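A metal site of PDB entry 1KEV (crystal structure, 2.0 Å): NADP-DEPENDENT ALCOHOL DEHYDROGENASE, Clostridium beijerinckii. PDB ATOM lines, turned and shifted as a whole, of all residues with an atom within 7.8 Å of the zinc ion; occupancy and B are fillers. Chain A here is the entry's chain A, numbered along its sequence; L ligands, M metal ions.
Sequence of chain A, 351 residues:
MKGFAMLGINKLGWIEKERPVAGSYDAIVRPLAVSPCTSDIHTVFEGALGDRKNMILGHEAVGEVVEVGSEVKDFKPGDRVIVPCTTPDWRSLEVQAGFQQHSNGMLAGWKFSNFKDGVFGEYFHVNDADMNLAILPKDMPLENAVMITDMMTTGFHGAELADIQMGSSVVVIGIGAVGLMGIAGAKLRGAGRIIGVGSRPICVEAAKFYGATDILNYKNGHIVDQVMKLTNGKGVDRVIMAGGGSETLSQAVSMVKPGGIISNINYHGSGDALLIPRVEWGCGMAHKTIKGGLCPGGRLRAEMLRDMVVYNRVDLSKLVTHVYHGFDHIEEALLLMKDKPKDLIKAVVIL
OG1 of Thr 38 sits close to O10 of the ligand. The backbone NH (N) of Val 178 lies within hydrogen-bond range of an oxygen (O9) of the ligand, 3.4 Å away.
The side-chain carboxylate (OE1) of Glu 60 lies within salt-bridge range of the side-chain amino group (NZ) of Lys 346, at 3.1 Å. The side-chain sulfur (SG) of Cys 85 is in hydrogen-bond range of the side-chain carboxylate (OD1) of Asp 150. The backbone NH (N) of Ser 35 sits at hydrogen-bond distance from the backbone carbonyl oxygen (O) of Glu 60, at 3.3 Å. ND1 of His 59 is in hydrogen-bond range of OG of Ser 113. The backbone carbonyl oxygen of Asp 150 is in hydrogen-bond range of the side-chain hydroxyl of Thr 154 (3.0 Å). The side-chain sulfur (SG) of Cys 37 lies close to the side-chain hydroxyl (OG) of Ser 39, 2.8 Å away.
Merely in contact with the zinc ion: Ser 39 (3.2 Å) and Glu 60 (3.6 Å). Within 4 Å of the zinc ion: Cys 37, Ser 39, His 59, Glu 60 and Asp 150.
The zinc ion is bound by NE2 of His 59 (2.0 Å). OD2 of Asp 150 is bound to the zinc ion. The zinc ion is bound by SG of Cys 37 (2.2 Å). The zinc ion has three donor atoms within binding distance.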
ATOM      1  N   SER A  35      12.838   8.478 -19.813  1.00  0.00           N
ATOM      2  CA  SER A  35      13.787   9.556 -20.131  1.00  0.00           C
ATOM      3  C   SER A  35      14.148   9.589 -21.621  1.00  0.00           C
ATOM      4  O   SER A  35      14.220   8.545 -22.280  1.00  0.00           O
ATOM      5  CB  SER A  35      15.047   9.407 -19.284  1.00  0.00           C
ATOM      6  OG  SER A  35      16.034  10.372 -19.624  1.00  0.00           O
ATOM      7  N   PRO A  36      14.313  10.804 -22.186  1.00  0.00           N
ATOM      8  CA  PRO A  36      14.687  10.994 -23.605  1.00  0.00           C
ATOM      9  C   PRO A  36      16.200  10.886 -23.830  1.00  0.00           C
ATOM     10  O   PRO A  36      16.991  11.176 -22.923  1.00  0.00           O
ATOM     11  CB  PRO A  36      14.157  12.399 -23.897  1.00  0.00           C
ATOM     12  CG  PRO A  36      14.352  13.099 -22.593  1.00  0.00           C
ATOM     13  CD  PRO A  36      13.869  12.076 -21.600  1.00  0.00           C
ATOM     14  N   CYS A  37      16.609  10.511 -25.045  1.00  0.00           N
ATOM     15  CA  CYS A  37      18.033  10.353 -25.369  1.00  0.00           C
ATOM     16  C   CYS A  37      18.478  11.096 -26.627  1.00  0.00           C
ATOM     17  O   CYS A  37      17.691  11.291 -27.561  1.00  0.00           O
ATOM     18  CB  CYS A  37      18.345   8.854 -25.524  1.00  0.00           C
ATOM     19  SG  CYS A  37      20.107   8.399 -25.720  1.00  0.00           S
ATOM     20  N   THR A  38      19.768  11.464 -26.679  1.00  0.00           N
ATOM     21  CA  THR A  38      20.340  12.146 -27.836  1.00  0.00           C
ATOM     22  C   THR A  38      20.271  11.256 -29.083  1.00  0.00           C
ATOM     23  O   THR A  38      20.294  11.746 -30.210  1.00  0.00           O
ATOM     24  CB  THR A  38      21.815  12.557 -27.598  1.00  0.00           C
ATOM     25  OG1 THR A  38      22.565  11.416 -27.167  1.00  0.00           O
ATOM     26  CG2 THR A  38      21.905  13.634 -26.538  1.00  0.00           C
ATOM     27  N   SER A  39      20.204   9.935 -28.865  1.00  0.00           N
ATOM     28  CA  SER A  39      20.105   8.982 -29.976  1.00  0.00           C
ATOM     29  C   SER A  39      18.832   9.252 -30.771  1.00  0.00           C
ATOM     30  O   SER A  39      18.846   9.209 -31.996  1.00  0.00           O
ATOM     31  CB  SER A  39      20.048   7.530 -29.504  1.00  0.00           C
ATOM     32  OG  SER A  39      20.636   7.317 -28.230  1.00  0.00           O
ATOM     33  N   ASP A  40      17.736   9.526 -30.055  1.00  0.00           N
ATOM     34  CA  ASP A  40      16.437   9.797 -30.687  1.00  0.00           C
ATOM     35  C   ASP A  40      16.528  11.031 -31.602  1.00  0.00           C
ATOM     36  O   ASP A  40      15.874  11.089 -32.643  1.00  0.00           O
ATOM     37  CB  ASP A  40      15.344  10.048 -29.619  1.00  0.00           C
ATOM     38  CG  ASP A  40      14.951   8.782 -28.849  1.00  0.00           C
ATOM     39  OD1 ASP A  40      14.847   7.704 -29.472  1.00  0.00           O
ATOM     40  OD2 ASP A  40      14.711   8.888 -27.625  1.00  0.00           O
ATOM     41  N   GLY A  58      11.693   6.350 -27.660  1.00  0.00           N
ATOM     42  CA  GLY A  58      12.081   6.004 -26.287  1.00  0.00           C
ATOM     43  C   GLY A  58      12.640   4.611 -26.044  1.00  0.00           C
ATOM     44  O   GLY A  58      12.144   3.626 -26.591  1.00  0.00           O
ATOM     45  N   HIS A  59      13.668   4.536 -25.194  1.00  0.00           N
ATOM     46  CA  HIS A  59      14.285   3.258 -24.844  1.00  0.00           C
ATOM     47  C   HIS A  59      14.800   3.184 -23.399  1.00  0.00           C
ATOM     48  O   HIS A  59      15.487   2.228 -23.031  1.00  0.00           O
ATOM     49  CB  HIS A  59      15.380   2.845 -25.844  1.00  0.00           C
ATOM     50  CG  HIS A  59      16.478   3.858 -26.048  1.00  0.00           C
ATOM     51  ND1 HIS A  59      16.606   4.623 -27.190  1.00  0.00           N
ATOM     52  CD2 HIS A  59      17.537   4.175 -25.274  1.00  0.00           C
ATOM     53  CE1 HIS A  59      17.722   5.376 -27.072  1.00  0.00           C
ATOM     54  NE2 HIS A  59      18.335   5.156 -25.921  1.00  0.00           N
ATOM     55  N   GLU A  60      14.455   4.173 -22.574  1.00  0.00           N
ATOM     56  CA  GLU A  60      14.892   4.194 -21.174  1.00  0.00           C
ATOM     57  C   GLU A  60      13.670   4.218 -20.248  1.00  0.00           C
ATOM     58  O   GLU A  60      12.973   5.242 -20.192  1.00  0.00           O
ATOM     59  CB  GLU A  60      15.763   5.425 -20.920  1.00  0.00           C
ATOM     60  CG  GLU A  60      17.050   5.439 -21.735  1.00  0.00           C
ATOM     61  CD  GLU A  60      17.795   6.742 -21.614  1.00  0.00           C
ATOM     62  OE1 GLU A  60      18.306   7.055 -20.522  1.00  0.00           O
ATOM     63  OE2 GLU A  60      17.874   7.466 -22.631  1.00  0.00           O
ATOM     64  N   CYS A  85      17.876  -1.109 -22.019  1.00  0.00           N
ATOM     65  CA  CYS A  85      17.630  -0.652 -23.394  1.00  0.00           C
ATOM     66  C   CYS A  85      17.920  -1.730 -24.433  1.00  0.00           C
ATOM     67  O   CYS A  85      17.268  -1.783 -25.493  1.00  0.00           O
ATOM     68  CB  CYS A  85      18.370   0.667 -23.706  1.00  0.00           C
ATOM     69  SG  CYS A  85      20.189   0.614 -23.828  1.00  0.00           S
ATOM     70  N   TRP A 110      19.454  -4.059 -29.823  1.00  0.00           N
ATOM     71  CA  TRP A 110      18.769  -2.831 -29.419  1.00  0.00           C
ATOM     72  C   TRP A 110      17.516  -2.724 -30.298  1.00  0.00           C
ATOM     73  O   TRP A 110      17.623  -2.484 -31.505  1.00  0.00           O
ATOM     74  CB  TRP A 110      19.705  -1.637 -29.619  1.00  0.00           C
ATOM     75  CG  TRP A 110      19.079  -0.300 -29.415  1.00  0.00           C
ATOM     76  CD1 TRP A 110      18.180   0.049 -28.446  1.00  0.00           C
ATOM     77  CD2 TRP A 110      19.296   0.866 -30.213  1.00  0.00           C
ATOM     78  NE1 TRP A 110      17.817   1.363 -28.598  1.00  0.00           N
ATOM     79  CE2 TRP A 110      18.486   1.890 -29.669  1.00  0.00           C
ATOM     80  CE3 TRP A 110      20.086   1.148 -31.335  1.00  0.00           C
ATOM     81  CZ2 TRP A 110      18.450   3.187 -30.215  1.00  0.00           C
ATOM     82  CZ3 TRP A 110      20.049   2.434 -31.873  1.00  0.00           C
ATOM     83  CH2 TRP A 110      19.235   3.435 -31.312  1.00  0.00           C
ATOM     84  N   SER A 113      12.847   1.924 -30.255  1.00  0.00           N
ATOM     85  CA  SER A 113      13.146   3.111 -31.067  1.00  0.00           C
ATOM     86  C   SER A 113      14.273   2.926 -32.099  1.00  0.00           C
ATOM     87  O   SER A 113      14.937   3.894 -32.495  1.00  0.00           O
ATOM     88  CB  SER A 113      13.395   4.373 -30.201  1.00  0.00           C
ATOM     89  OG  SER A 113      14.690   4.418 -29.623  1.00  0.00           O
ATOM     90  N   THR A 149      19.354   1.832 -17.140  1.00  0.00           N
ATOM     91  CA  THR A 149      18.925   1.308 -18.438  1.00  0.00           C
ATOM     92  C   THR A 149      19.791   1.663 -19.650  1.00  0.00           C
ATOM     93  O   THR A 149      19.765   0.951 -20.659  1.00  0.00           O
ATOM     94  CB  THR A 149      17.442   1.683 -18.721  1.00  0.00           C
ATOM     95  OG1 THR A 149      17.313   3.103 -18.846  1.00  0.00           O
ATOM     96  CG2 THR A 149      16.544   1.233 -17.573  1.00  0.00           C
ATOM     97  N   ASP A 150      20.542   2.759 -19.591  1.00  0.00           N
ATOM     98  CA  ASP A 150      21.358   3.153 -20.737  1.00  0.00           C
ATOM     99  C   ASP A 150      22.646   3.926 -20.423  1.00  0.00           C
ATOM    100  O   ASP A 150      23.728   3.503 -20.830  1.00  0.00           O
ATOM    101  CB  ASP A 150      20.482   3.949 -21.707  1.00  0.00           C
ATOM    102  CG  ASP A 150      21.195   4.305 -23.009  1.00  0.00           C
ATOM    103  OD1 ASP A 150      22.162   3.626 -23.402  1.00  0.00           O
ATOM    104  OD2 ASP A 150      20.742   5.274 -23.656  1.00  0.00           O
ATOM    105  N   MET A 151      22.541   5.025 -19.698  1.00  0.00           N
ATOM    106  CA  MET A 151      23.714   5.841 -19.387  1.00  0.00           C
ATOM    107  C   MET A 151      24.814   5.072 -18.654  1.00  0.00           C
ATOM    108  O   MET A 151      25.978   5.080 -19.074  1.00  0.00           O
ATOM    109  CB  MET A 151      23.320   7.090 -18.594  1.00  0.00           C
ATOM    110  CG  MET A 151      22.308   8.026 -19.298  1.00  0.00           C
ATOM    111  SD  MET A 151      22.888   8.758 -20.852  1.00  0.00           S
ATOM    112  CE  MET A 151      22.173   7.688 -22.027  1.00  0.00           C
ATOM    113  N   THR A 154      26.328   2.103 -20.837  1.00  0.00           N
ATOM    114  CA  THR A 154      27.107   2.610 -21.959  1.00  0.00           C
ATOM    115  C   THR A 154      28.459   3.204 -21.525  1.00  0.00           C
ATOM    116  O   THR A 154      29.509   2.854 -22.080  1.00  0.00           O
ATOM    117  CB  THR A 154      26.320   3.621 -22.800  1.00  0.00           C
ATOM    118  OG1 THR A 154      25.167   2.989 -23.371  1.00  0.00           O
ATOM    119  CG2 THR A 154      27.179   4.213 -23.920  1.00  0.00           C
ATOM    120  N   VAL A 178      26.800  10.305 -21.011  1.00  0.00           N
ATOM    121  CA  VAL A 178      27.603   9.128 -21.332  1.00  0.00           C
ATOM    122  C   VAL A 178      29.083   9.307 -20.952  1.00  0.00           C
ATOM    123  O   VAL A 178      29.698   8.408 -20.379  1.00  0.00           O
ATOM    124  CB  VAL A 178      27.486   8.769 -22.819  1.00  0.00           C
ATOM    125  CG1 VAL A 178      28.365   7.585 -23.170  1.00  0.00           C
ATOM    126  CG2 VAL A 178      26.061   8.448 -23.129  1.00  0.00           C
ATOM    127  N   CYS A 295      26.244  -0.875 -26.062  1.00  0.00           N
ATOM    128  CA  CYS A 295      26.119  -1.325 -24.664  1.00  0.00           C
ATOM    129  C   CYS A 295      25.416  -2.665 -24.467  1.00  0.00           C
ATOM    130  O   CYS A 295      24.497  -3.006 -25.219  1.00  0.00           O
ATOM    131  CB  CYS A 295      25.393  -0.258 -23.829  1.00  0.00           C
ATOM    132  SG  CYS A 295      23.592  -0.139 -24.142  1.00  0.00           S
ATOM    133  N   LYS A 346      20.416  15.184 -17.850  1.00  0.00           N
ATOM    134  CA  LYS A 346      19.345  14.210 -18.136  1.00  0.00           C
ATOM    135  C   LYS A 346      18.011  14.646 -17.503  1.00  0.00           C
ATOM    136  O   LYS A 346      17.998  15.295 -16.443  1.00  0.00           O
ATOM    137  CB  LYS A 346      19.705  12.803 -17.644  1.00  0.00           C
ATOM    138  CG  LYS A 346      20.788  12.091 -18.464  1.00  0.00           C
ATOM    139  CD  LYS A 346      20.329  11.698 -19.865  1.00  0.00           C
ATOM    140  CE  LYS A 346      19.500  10.436 -19.866  1.00  0.00           C
ATOM    141  NZ  LYS A 346      19.261   9.941 -21.251  1.00  0.00           N
HETATM  142  P1  LIG L   1      25.711  15.177 -25.339  1.00  0.00           P
HETATM  143  O1  LIG L   1      25.035  15.782 -26.511  1.00  0.00           O
HETATM  144  O2  LIG L   1      25.265  15.619 -24.006  1.00  0.00           O
HETATM  145  O3  LIG L   1      27.211  15.806 -25.460  1.00  0.00           O
HETATM  146  C1  LIG L   1      28.409  15.365 -24.792  1.00  0.00           C
HETATM  147  C2  LIG L   1      29.671  16.209 -25.009  1.00  0.00           C
HETATM  148  O4  LIG L   1      29.971  16.465 -26.404  1.00  0.00           O
HETATM  149  C3  LIG L   1      29.607  17.541 -24.248  1.00  0.00           C
HETATM  150  O5  LIG L   1      30.343  17.442 -23.028  1.00  0.00           O
HETATM  151  C4  LIG L   1      30.420  18.468 -25.132  1.00  0.00           C
HETATM  152  O6  LIG L   1      30.806  19.836 -24.858  1.00  0.00           O
HETATM  153  C5  LIG L   1      30.611  17.754 -26.444  1.00  0.00           C
HETATM  154  N1  LIG L   1      31.438  18.252 -27.579  1.00  0.00           N
HETATM  155  C6  LIG L   1      30.972  18.863 -28.686  1.00  0.00           C
HETATM  156  N2  LIG L   1      31.906  18.965 -29.637  1.00  0.00           N
HETATM  157  C7  LIG L   1      32.966  18.399 -29.070  1.00  0.00           C
HETATM  158  C8  LIG L   1      34.201  18.256 -29.701  1.00  0.00           C
HETATM  159  N3  LIG L   1      34.374  18.677 -30.948  1.00  0.00           N
HETATM  160  N4  LIG L   1      35.167  17.669 -28.956  1.00  0.00           N
HETATM  161  C9  LIG L   1      34.944  17.250 -27.704  1.00  0.00           C
HETATM  162  N5  LIG L   1      33.749  17.374 -27.114  1.00  0.00           N
HETATM  163  C10 LIG L   1      32.725  17.955 -27.784  1.00  0.00           C
HETATM  164  O7  LIG L   1      25.725  13.568 -25.409  1.00  0.00           O
HETATM  165  P2  LIG L   1      25.921  12.208 -24.518  1.00  0.00           P
HETATM  166  O8  LIG L   1      24.674  11.934 -23.758  1.00  0.00           O
HETATM  167  O9  LIG L   1      27.265  12.075 -23.918  1.00  0.00           O
HETATM  168  O10 LIG L   1      25.650  11.096 -25.689  1.00  0.00           O
HETATM  169  C11 LIG L   1      26.862  10.622 -26.375  1.00  0.00           C
HETATM  170  C12 LIG L   1      27.066   9.638 -27.569  1.00  0.00           C
HETATM  171  O11 LIG L   1      26.883   8.254 -27.165  1.00  0.00           O
HETATM  172  C13 LIG L   1      25.961  10.188 -28.491  1.00  0.00           C
HETATM  173  O12 LIG L   1      26.159  10.022 -29.876  1.00  0.00           O
HETATM  174  C14 LIG L   1      24.865   9.207 -28.062  1.00  0.00           C
HETATM  175  O13 LIG L   1      23.877   8.832 -29.090  1.00  0.00           O
HETATM  176  C15 LIG L   1      25.687   7.917 -27.744  1.00  0.00           C
HETATM  177  N6  LIG L   1      24.885   6.903 -27.023  1.00  0.00           N
HETATM  178  C16 LIG L   1      24.159   5.844 -27.694  1.00  0.00           C
HETATM  179  C17 LIG L   1      23.168   5.155 -27.007  1.00  0.00           C
HETATM  180  C18 LIG L   1      22.411   3.951 -27.582  1.00  0.00           C
HETATM  181  O14 LIG L   1      21.975   3.025 -26.889  1.00  0.00           O
HETATM  182  N7  LIG L   1      22.262   4.011 -28.907  1.00  0.00           N
HETATM  183  C19 LIG L   1      22.993   5.544 -25.674  1.00  0.00           C
HETATM  184  C20 LIG L   1      23.700   6.530 -24.996  1.00  0.00           C
HETATM  185  C21 LIG L   1      24.671   7.229 -25.663  1.00  0.00           C
HETATM  186  P3  LIG L   1      30.045  20.808 -23.812  1.00  0.00           P
HETATM  187  O15 LIG L   1      30.534  22.140 -24.222  1.00  0.00           O
HETATM  188  O16 LIG L   1      30.529  20.403 -22.460  1.00  0.00           O
HETATM  189  O17 LIG L   1      28.600  20.573 -24.070  1.00  0.00           O
HETATM  190 ZN    ZN M   1      19.925   6.193 -25.344  1.00  0.00          ZN
